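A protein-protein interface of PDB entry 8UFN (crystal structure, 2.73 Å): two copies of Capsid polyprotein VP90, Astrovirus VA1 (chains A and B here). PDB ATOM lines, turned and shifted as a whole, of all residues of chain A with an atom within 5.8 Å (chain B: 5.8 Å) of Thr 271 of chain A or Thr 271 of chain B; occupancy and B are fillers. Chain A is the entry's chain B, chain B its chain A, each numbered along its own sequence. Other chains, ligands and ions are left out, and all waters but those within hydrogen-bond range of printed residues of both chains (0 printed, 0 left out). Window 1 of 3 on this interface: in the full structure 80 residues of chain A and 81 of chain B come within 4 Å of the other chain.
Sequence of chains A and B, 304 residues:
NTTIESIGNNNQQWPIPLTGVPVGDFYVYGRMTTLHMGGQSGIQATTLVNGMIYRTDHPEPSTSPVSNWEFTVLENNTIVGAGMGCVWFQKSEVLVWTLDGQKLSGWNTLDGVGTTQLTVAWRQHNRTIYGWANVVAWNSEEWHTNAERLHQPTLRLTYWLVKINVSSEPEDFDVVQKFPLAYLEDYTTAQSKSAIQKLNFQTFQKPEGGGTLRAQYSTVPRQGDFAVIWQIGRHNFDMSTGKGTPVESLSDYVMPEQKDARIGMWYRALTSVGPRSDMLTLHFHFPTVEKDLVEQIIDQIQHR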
ATOM      1  N   VAL A  49      -3.573   1.562  32.630  1.00  0.00           N
ATOM      2  CA  VAL A  49      -2.309   2.287  32.632  1.00  0.00           C
ATOM      3  C   VAL A  49      -2.284   3.435  31.623  1.00  0.00           C
ATOM      4  O   VAL A  49      -1.536   4.400  31.808  1.00  0.00           O
ATOM      5  CB  VAL A  49      -1.152   1.301  32.383  1.00  0.00           C
ATOM      6  CG1 VAL A  49      -1.103   0.882  30.917  1.00  0.00           C
ATOM      7  CG2 VAL A  49       0.171   1.903  32.822  1.00  0.00           C
ATOM      8  N   ASN A  50      -3.091   3.368  30.564  1.00  0.00           N
ATOM      9  CA  ASN A  50      -2.987   4.352  29.495  1.00  0.00           C
ATOM     10  C   ASN A  50      -4.233   5.221  29.387  1.00  0.00           C
ATOM     11  O   ASN A  50      -4.922   5.206  28.362  1.00  0.00           O
ATOM     12  CB  ASN A  50      -2.714   3.657  28.160  1.00  0.00           C
ATOM     13  CG  ASN A  50      -1.278   3.816  27.706  1.00  0.00           C
ATOM     14  OD1 ASN A  50      -0.473   4.467  28.372  1.00  0.00           O
ATOM     15  ND2 ASN A  50      -0.948   3.218  26.568  1.00  0.00           N
ATOM     16  N   PHE A 179      -8.419   5.594  25.495  1.00  0.00           N
ATOM     17  CA  PHE A 179      -7.470   4.520  25.742  1.00  0.00           C
ATOM     18  C   PHE A 179      -7.063   3.862  24.430  1.00  0.00           C
ATOM     19  O   PHE A 179      -7.813   3.897  23.449  1.00  0.00           O
ATOM     20  CB  PHE A 179      -8.079   3.459  26.670  1.00  0.00           C
ATOM     21  CG  PHE A 179      -7.999   3.803  28.131  1.00  0.00           C
ATOM     22  CD1 PHE A 179      -8.702   4.879  28.646  1.00  0.00           C
ATOM     23  CD2 PHE A 179      -7.229   3.037  28.992  1.00  0.00           C
ATOM     24  CE1 PHE A 179      -8.632   5.189  29.990  1.00  0.00           C
ATOM     25  CE2 PHE A 179      -7.153   3.343  30.335  1.00  0.00           C
ATOM     26  CZ  PHE A 179      -7.859   4.419  30.837  1.00  0.00           C
ATOM     27  N   PRO A 180      -5.882   3.247  24.379  1.00  0.00           N
ATOM     28  CA  PRO A 180      -5.502   2.443  23.218  1.00  0.00           C
ATOM     29  C   PRO A 180      -5.983   1.007  23.354  1.00  0.00           C
ATOM     30  O   PRO A 180      -6.061   0.444  24.448  1.00  0.00           O
ATOM     31  CB  PRO A 180      -3.965   2.506  23.240  1.00  0.00           C
ATOM     32  CG  PRO A 180      -3.589   3.103  24.597  1.00  0.00           C
ATOM     33  CD  PRO A 180      -4.840   3.202  25.412  1.00  0.00           C
ATOM     34  N   TRP A 266       6.386   1.813  21.890  1.00  0.00           N
ATOM     35  CA  TRP A 266       5.096   1.662  21.224  1.00  0.00           C
ATOM     36  C   TRP A 266       4.149   0.796  22.042  1.00  0.00           C
ATOM     37  O   TRP A 266       2.955   1.100  22.150  1.00  0.00           O
ATOM     38  CB  TRP A 266       5.293   1.071  19.831  1.00  0.00           C
ATOM     39  CG  TRP A 266       5.721   2.074  18.812  1.00  0.00           C
ATOM     40  CD1 TRP A 266       6.994   2.497  18.562  1.00  0.00           C
ATOM     41  CD2 TRP A 266       4.877   2.784  17.898  1.00  0.00           C
ATOM     42  NE1 TRP A 266       6.995   3.424  17.549  1.00  0.00           N
ATOM     43  CE2 TRP A 266       5.708   3.619  17.124  1.00  0.00           C
ATOM     44  CE3 TRP A 266       3.500   2.792  17.657  1.00  0.00           C
ATOM     45  CZ2 TRP A 266       5.206   4.455  16.129  1.00  0.00           C
ATOM     46  CZ3 TRP A 266       3.004   3.624  16.670  1.00  0.00           C
ATOM     47  CH2 TRP A 266       3.855   4.443  15.917  1.00  0.00           C
ATOM     48  N   TYR A 267       4.661  -0.290  22.627  1.00  0.00           N
ATOM     49  CA  TYR A 267       3.807  -1.187  23.397  1.00  0.00           C
ATOM     50  C   TYR A 267       3.297  -0.514  24.665  1.00  0.00           C
ATOM     51  O   TYR A 267       2.148  -0.727  25.066  1.00  0.00           O
ATOM     52  CB  TYR A 267       4.567  -2.471  23.728  1.00  0.00           C
ATOM     53  CG  TYR A 267       5.122  -3.156  22.502  1.00  0.00           C
ATOM     54  CD1 TYR A 267       4.306  -3.437  21.414  1.00  0.00           C
ATOM     55  CD2 TYR A 267       6.464  -3.505  22.424  1.00  0.00           C
ATOM     56  CE1 TYR A 267       4.807  -4.057  20.289  1.00  0.00           C
ATOM     57  CE2 TYR A 267       6.974  -4.127  21.300  1.00  0.00           C
ATOM     58  CZ  TYR A 267       6.141  -4.400  20.236  1.00  0.00           C
ATOM     59  OH  TYR A 267       6.639  -5.018  19.113  1.00  0.00           O
ATOM     60  N   ARG A 268       4.132   0.307  25.305  1.00  0.00           N
ATOM     61  CA  ARG A 268       3.670   1.065  26.464  1.00  0.00           C
ATOM     62  C   ARG A 268       2.625   2.098  26.060  1.00  0.00           C
ATOM     63  O   ARG A 268       1.661   2.336  26.795  1.00  0.00           O
ATOM     64  CB  ARG A 268       4.860   1.733  27.156  1.00  0.00           C
ATOM     65  CG  ARG A 268       4.483   2.813  28.159  1.00  0.00           C
ATOM     66  CD  ARG A 268       4.062   2.211  29.492  1.00  0.00           C
ATOM     67  NE  ARG A 268       3.318   3.156  30.318  1.00  0.00           N
ATOM     68  CZ  ARG A 268       2.080   3.566  30.068  1.00  0.00           C
ATOM     69  NH1 ARG A 268       1.404   3.124  29.020  1.00  0.00           N
ATOM     70  NH2 ARG A 268       1.506   4.435  30.893  1.00  0.00           N
ATOM     71  N   ALA A 269       2.792   2.710  24.887  1.00  0.00           N
ATOM     72  CA  ALA A 269       1.852   3.714  24.405  1.00  0.00           C
ATOM     73  C   ALA A 269       0.595   3.114  23.786  1.00  0.00           C
ATOM     74  O   ALA A 269      -0.364   3.851  23.539  1.00  0.00           O
ATOM     75  CB  ALA A 269       2.536   4.624  23.381  1.00  0.00           C
ATOM     76  N   LEU A 270       0.574   1.805  23.532  1.00  0.00           N
ATOM     77  CA  LEU A 270      -0.585   1.145  22.946  1.00  0.00           C
ATOM     78  C   LEU A 270      -1.241   0.141  23.881  1.00  0.00           C
ATOM     79  O   LEU A 270      -2.309  -0.384  23.547  1.00  0.00           O
ATOM     80  CB  LEU A 270      -0.188   0.441  21.641  1.00  0.00           C
ATOM     81  CG  LEU A 270       0.127   1.373  20.470  1.00  0.00           C
ATOM     82  CD1 LEU A 270       1.083   0.701  19.499  1.00  0.00           C
ATOM     83  CD2 LEU A 270      -1.151   1.803  19.767  1.00  0.00           C
ATOM     84  N   THR A 271      -0.635  -0.137  25.031  1.00  0.00           N
ATOM     85  CA  THR A 271      -1.193  -1.092  25.978  1.00  0.00           C
ATOM     86  C   THR A 271      -2.498  -0.565  26.564  1.00  0.00           C
ATOM     87  O   THR A 271      -2.624   0.619  26.882  1.00  0.00           O
ATOM     88  CB  THR A 271      -0.179  -1.369  27.091  1.00  0.00           C
ATOM     89  OG1 THR A 271       0.773  -2.342  26.646  1.00  0.00           O
ATOM     90  CG2 THR A 271      -0.860  -1.878  28.341  1.00  0.00           C
ATOM     91  N   SER A 272      -3.485  -1.458  26.693  1.00  0.00           N
ATOM     92  CA  SER A 272      -4.747  -1.076  27.318  1.00  0.00           C
ATOM     93  C   SER A 272      -4.675  -1.177  28.839  1.00  0.00           C
ATOM     94  O   SER A 272      -5.204  -0.310  29.545  1.00  0.00           O
ATOM     95  CB  SER A 272      -5.885  -1.945  26.784  1.00  0.00           C
ATOM     96  OG  SER A 272      -6.013  -1.811  25.379  1.00  0.00           O
ATOM     97  N   VAL A 273      -4.025  -2.215  29.361  1.00  0.00           N
ATOM     98  CA  VAL A 273      -3.964  -2.464  30.798  1.00  0.00           C
ATOM     99  C   VAL A 273      -2.557  -2.907  31.172  1.00  0.00           C
ATOM    100  O   VAL A 273      -1.976  -3.772  30.511  1.00  0.00           O
ATOM    101  CB  VAL A 273      -4.988  -3.526  31.241  1.00  0.00           C
ATOM    102  CG1 VAL A 273      -6.366  -2.917  31.352  1.00  0.00           C
ATOM    103  CG2 VAL A 273      -4.992  -4.694  30.268  1.00  0.00           C
ATOM    104  N   GLY A 274      -2.019  -2.330  32.243  1.00  0.00           N
ATOM    105  CA  GLY A 274      -0.702  -2.686  32.712  1.00  0.00           C
ATOM    106  C   GLY A 274      -0.467  -2.275  34.151  1.00  0.00           C
ATOM    107  O   GLY A 274      -1.306  -1.626  34.784  1.00  0.00           O
ATOM    108  N   VAL B  49      -0.317  -7.937  17.887  1.00  0.00           N
ATOM    109  CA  VAL B  49       1.035  -8.332  18.265  1.00  0.00           C
ATOM    110  C   VAL B  49       1.047  -9.414  19.347  1.00  0.00           C
ATOM    111  O   VAL B  49       2.009 -10.186  19.434  1.00  0.00           O
ATOM    112  CB  VAL B  49       1.829  -7.086  18.701  1.00  0.00           C
ATOM    113  CG1 VAL B  49       1.254  -6.495  19.983  1.00  0.00           C
ATOM    114  CG2 VAL B  49       3.311  -7.409  18.850  1.00  0.00           C
ATOM    115  N   ASN B  50      -0.001  -9.510  20.160  1.00  0.00           N
ATOM    116  CA  ASN B  50      -0.030 -10.436  21.290  1.00  0.00           C
ATOM    117  C   ASN B  50      -0.987 -11.588  20.992  1.00  0.00           C
ATOM    118  O   ASN B  50      -2.089 -11.672  21.541  1.00  0.00           O
ATOM    119  CB  ASN B  50      -0.425  -9.696  22.568  1.00  0.00           C
ATOM    120  CG  ASN B  50       0.670  -9.715  23.614  1.00  0.00           C
ATOM    121  OD1 ASN B  50       1.401 -10.699  23.744  1.00  0.00           O
ATOM    122  ND2 ASN B  50       0.795  -8.625  24.361  1.00  0.00           N
ATOM    123  N   PHE B 179      -5.867 -13.141  23.733  1.00  0.00           N
ATOM    124  CA  PHE B 179      -5.394 -11.763  23.644  1.00  0.00           C
ATOM    125  C   PHE B 179      -5.690 -11.023  24.944  1.00  0.00           C
ATOM    126  O   PHE B 179      -6.810 -11.136  25.476  1.00  0.00           O
ATOM    127  CB  PHE B 179      -6.048 -11.037  22.465  1.00  0.00           C
ATOM    128  CG  PHE B 179      -5.274 -11.133  21.181  1.00  0.00           C
ATOM    129  CD1 PHE B 179      -5.247 -12.313  20.457  1.00  0.00           C
ATOM    130  CD2 PHE B 179      -4.584 -10.037  20.691  1.00  0.00           C
ATOM    131  CE1 PHE B 179      -4.540 -12.401  19.274  1.00  0.00           C
ATOM    132  CE2 PHE B 179      -3.876 -10.118  19.507  1.00  0.00           C
ATOM    133  CZ  PHE B 179      -3.853 -11.302  18.798  1.00  0.00           C
ATOM    134  N   PRO B 180      -4.733 -10.265  25.474  1.00  0.00           N
ATOM    135  CA  PRO B 180      -4.983  -9.468  26.677  1.00  0.00           C
ATOM    136  C   PRO B 180      -5.570  -8.105  26.349  1.00  0.00           C
ATOM    137  O   PRO B 180      -5.298  -7.511  25.305  1.00  0.00           O
ATOM    138  CB  PRO B 180      -3.584  -9.324  27.301  1.00  0.00           C
ATOM    139  CG  PRO B 180      -2.609  -9.967  26.314  1.00  0.00           C
ATOM    140  CD  PRO B 180      -3.340 -10.149  25.028  1.00  0.00           C
ATOM    141  N   TRP B 266       5.726  -6.422  31.187  1.00  0.00           N
ATOM    142  CA  TRP B 266       4.281  -6.455  31.392  1.00  0.00           C
ATOM    143  C   TRP B 266       3.530  -5.708  30.294  1.00  0.00           C
ATOM    144  O   TRP B 266       2.487  -6.177  29.827  1.00  0.00           O
ATOM    145  CB  TRP B 266       3.946  -5.879  32.765  1.00  0.00           C
ATOM    146  CG  TRP B 266       4.399  -6.750  33.893  1.00  0.00           C
ATOM    147  CD1 TRP B 266       5.652  -6.811  34.428  1.00  0.00           C
ATOM    148  CD2 TRP B 266       3.605  -7.691  34.625  1.00  0.00           C
ATOM    149  NE1 TRP B 266       5.689  -7.730  35.448  1.00  0.00           N
ATOM    150  CE2 TRP B 266       4.444  -8.285  35.587  1.00  0.00           C
ATOM    151  CE3 TRP B 266       2.268  -8.092  34.556  1.00  0.00           C
ATOM    152  CZ2 TRP B 266       3.989  -9.256  36.477  1.00  0.00           C
ATOM    153  CZ3 TRP B 266       1.817  -9.056  35.440  1.00  0.00           C
ATOM    154  CH2 TRP B 266       2.675  -9.626  36.388  1.00  0.00           C
ATOM    155  N   TYR B 267       4.038  -4.549  29.872  1.00  0.00           N
ATOM    156  CA  TYR B 267       3.322  -3.767  28.867  1.00  0.00           C
ATOM    157  C   TYR B 267       3.298  -4.477  27.519  1.00  0.00           C
ATOM    158  O   TYR B 267       2.276  -4.465  26.823  1.00  0.00           O
ATOM    159  CB  TYR B 267       3.948  -2.379  28.736  1.00  0.00           C
ATOM    160  CG  TYR B 267       4.033  -1.635  30.047  1.00  0.00           C
ATOM    161  CD1 TYR B 267       2.901  -1.434  30.827  1.00  0.00           C
ATOM    162  CD2 TYR B 267       5.243  -1.133  30.507  1.00  0.00           C
ATOM    163  CE1 TYR B 267       2.972  -0.756  32.028  1.00  0.00           C
ATOM    164  CE2 TYR B 267       5.324  -0.452  31.706  1.00  0.00           C
ATOM    165  CZ  TYR B 267       4.186  -0.266  32.463  1.00  0.00           C
ATOM    166  OH  TYR B 267       4.262   0.411  33.658  1.00  0.00           O
ATOM    167  N   ARG B 268       4.411  -5.107  27.137  1.00  0.00           N
ATOM    168  CA  ARG B 268       4.438  -5.840  25.877  1.00  0.00           C
ATOM    169  C   ARG B 268       3.611  -7.119  25.960  1.00  0.00           C
ATOM    170  O   ARG B 268       3.030  -7.548  24.955  1.00  0.00           O
ATOM    171  CB  ARG B 268       5.887  -6.143  25.484  1.00  0.00           C
ATOM    172  CG  ARG B 268       6.067  -7.289  24.502  1.00  0.00           C
ATOM    173  CD  ARG B 268       5.818  -6.849  23.075  1.00  0.00           C
ATOM    174  NE  ARG B 268       4.480  -7.217  22.631  1.00  0.00           N
ATOM    175  CZ  ARG B 268       4.158  -8.408  22.144  1.00  0.00           C
ATOM    176  NH1 ARG B 268       5.064  -9.359  21.989  1.00  0.00           N
ATOM    177  NH2 ARG B 268       2.896  -8.653  21.809  1.00  0.00           N
ATOM    178  N   ALA B 269       3.521  -7.724  27.143  1.00  0.00           N
ATOM    179  CA  ALA B 269       2.746  -8.948  27.311  1.00  0.00           C
ATOM    180  C   ALA B 269       1.256  -8.689  27.492  1.00  0.00           C
ATOM    181  O   ALA B 269       0.460  -9.623  27.347  1.00  0.00           O
ATOM    182  CB  ALA B 269       3.273  -9.748  28.504  1.00  0.00           C
ATOM    183  N   LEU B 270       0.861  -7.454  27.799  1.00  0.00           N
ATOM    184  CA  LEU B 270      -0.534  -7.130  28.062  1.00  0.00           C
ATOM    185  C   LEU B 270      -1.160  -6.236  27.001  1.00  0.00           C
ATOM    186  O   LEU B 270      -2.360  -5.955  27.079  1.00  0.00           O
ATOM    187  CB  LEU B 270      -0.671  -6.463  29.436  1.00  0.00           C
ATOM    188  CG  LEU B 270      -0.461  -7.371  30.648  1.00  0.00           C
ATOM    189  CD1 LEU B 270      -0.054  -6.555  31.865  1.00  0.00           C
ATOM    190  CD2 LEU B 270      -1.715  -8.181  30.934  1.00  0.00           C
ATOM    191  N   THR B 271      -0.389  -5.777  26.019  1.00  0.00           N
ATOM    192  CA  THR B 271      -0.959  -4.954  24.962  1.00  0.00           C
ATOM    193  C   THR B 271      -1.798  -5.810  24.019  1.00  0.00           C
ATOM    194  O   THR B 271      -1.416  -6.928  23.660  1.00  0.00           O
ATOM    195  CB  THR B 271       0.146  -4.233  24.184  1.00  0.00           C
ATOM    196  OG1 THR B 271      -0.433  -3.497  23.099  1.00  0.00           O
ATOM    197  CG2 THR B 271       1.173  -5.221  23.641  1.00  0.00           C
ATOM    198  N   SER B 272      -2.963  -5.287  23.640  1.00  0.00           N
ATOM    199  CA  SER B 272      -3.786  -5.977  22.656  1.00  0.00           C
ATOM    200  C   SER B 272      -3.278  -5.749  21.241  1.00  0.00           C
ATOM    201  O   SER B 272      -3.440  -6.618  20.378  1.00  0.00           O
ATOM    202  CB  SER B 272      -5.242  -5.523  22.765  1.00  0.00           C
ATOM    203  OG  SER B 272      -5.674  -5.503  24.114  1.00  0.00           O
ATOM    204  N   VAL B 273      -2.653  -4.598  20.994  1.00  0.00           N
ATOM    205  CA  VAL B 273      -2.186  -4.224  19.667  1.00  0.00           C
ATOM    206  C   VAL B 273      -0.820  -3.561  19.793  1.00  0.00           C
ATOM    207  O   VAL B 273      -0.417  -3.107  20.866  1.00  0.00           O
ATOM    208  CB  VAL B 273      -3.174  -3.277  18.955  1.00  0.00           C
ATOM    209  CG1 VAL B 273      -4.314  -4.066  18.334  1.00  0.00           C
ATOM    210  CG2 VAL B 273      -3.697  -2.233  19.929  1.00  0.00           C
ATOM    211  N   GLY B 274      -0.109  -3.510  18.671  1.00  0.00           N
ATOM    212  CA  GLY B 274       1.204  -2.914  18.629  1.00  0.00           C
ATOM    213  C   GLY B 274       1.967  -3.307  17.382  1.00  0.00           C
ATOM    214  O   GLY B 274       1.552  -4.192  16.627  1.00  0.00           O
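The side-chain hydroxyl (OG1) of Thr 271 of chain A is in hydrogen-bond range of the backbone carbonyl oxygen (O) of Tyr 267 of chain B (2.6 Å).
The backbone carbonyl oxygen of Val 49 of chain A is in hydrogen-bond range of the guanidinium group of Arg 268 of chain A, 3.2 Å away. The side-chain amide nitrogen (ND2) of Asn 50 of chain B is in hydrogen-bond range of the backbone carbonyl oxygen (O) of Arg 268 of chain B, 2.6 Å away. O of Thr 271 of chain A sits at hydrogen-bond distance from ND2 of Asn 50 of chain A (3.1 Å). The side-chain amide nitrogen of Asn 50 of chain B is in hydrogen-bond range of the backbone carbonyl oxygen of Thr 271 of chain B (2.9 Å). The backbone carbonyl oxygen (O) of Pro 180 of chain A sits at hydrogen-bond distance from the side-chain hydroxyl (OG) of Ser 272 of chain A (2.4 Å). O of Val 49 of chain B is in hydrogen-bond range of NH2 of Arg 268 of chain B, 3.0 Å away.
Among the printed residues, pairs that only touch across the chains: Val 49 of chain A with Tyr 267 of chain B (3.9 Å), Tyr 267 of chain A with Val 49 of chain B (3.9 Å), Tyr 267 of chain A with Arg 268 of chain B (3.4 Å), Arg 268 of chain A with Tyr 267 of chain B (3.7 Å), Leu 270 of chain A with Thr 271 of chain B (3.7 Å), Leu 270 of chain A with Val 273 of chain B (3.6 Å), Leu 270 of chain A with Gly 274 of chain B (3.7 Å), Thr 271 of chain A with Thr 271 of chain B (3.2 Å), Ser 272 of chain A with Ser 272 of chain B (3.9 Å) and Val 273 of chain A with Leu 270 of chain B (3.2 Å).
Thr 271 of chain A touches just these residues of chain B: Tyr 267 and Thr 271. Of the printed residues of chain B, Ser 272 of chain A touches Ser 272 (3.9 Å). Asn 50 of chain B touches none of the printed residues of chain A. Thr 271 of chain B touches two residues of chain A. Of the printed residues of chain A, Gly 274 of chain B touches Leu 270. The nearest residue of chain B that does not touch Thr 271 of chain A is Leu 270 of chain B (4.4 Å).
Hydrophobic or aromatic side chains of chain A that line the printed part of chain B: Val 49, Tyr 267 and Leu 270. Printed residues of chain B that touch a printed residue of chain A: Val 49, Tyr 267, Arg 268, Leu 270, Thr 271, Ser 272, Val 273 and Gly 274. Hydrophobic or aromatic side chains of chain B within 4 Å of the printed part of chain A: Val 49, Tyr 267 and Leu 270. Among the printed residues, 11 pairs touch across the chains. Among the printed residues, no Asp or Glu carboxylate lies within 4 Å of a Lys or Arg side-chain nitrogen of the other chain.
Val 49 of chain A touches Tyr 267 of chain B, and with the chains exchanged Tyr 267 of chain A touches Val 49 of chain B. Thr 271 of chain A touches Tyr 267 of chain B, but with the chains exchanged Tyr 267 of chain A does not touch Thr 271 of chain B (4.1 Å). Thr 271 of chain B touches its own counterpart, Thr 271 of chain A. Ser 272 of chain B touches its own counterpart, Ser 272 of chain A.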
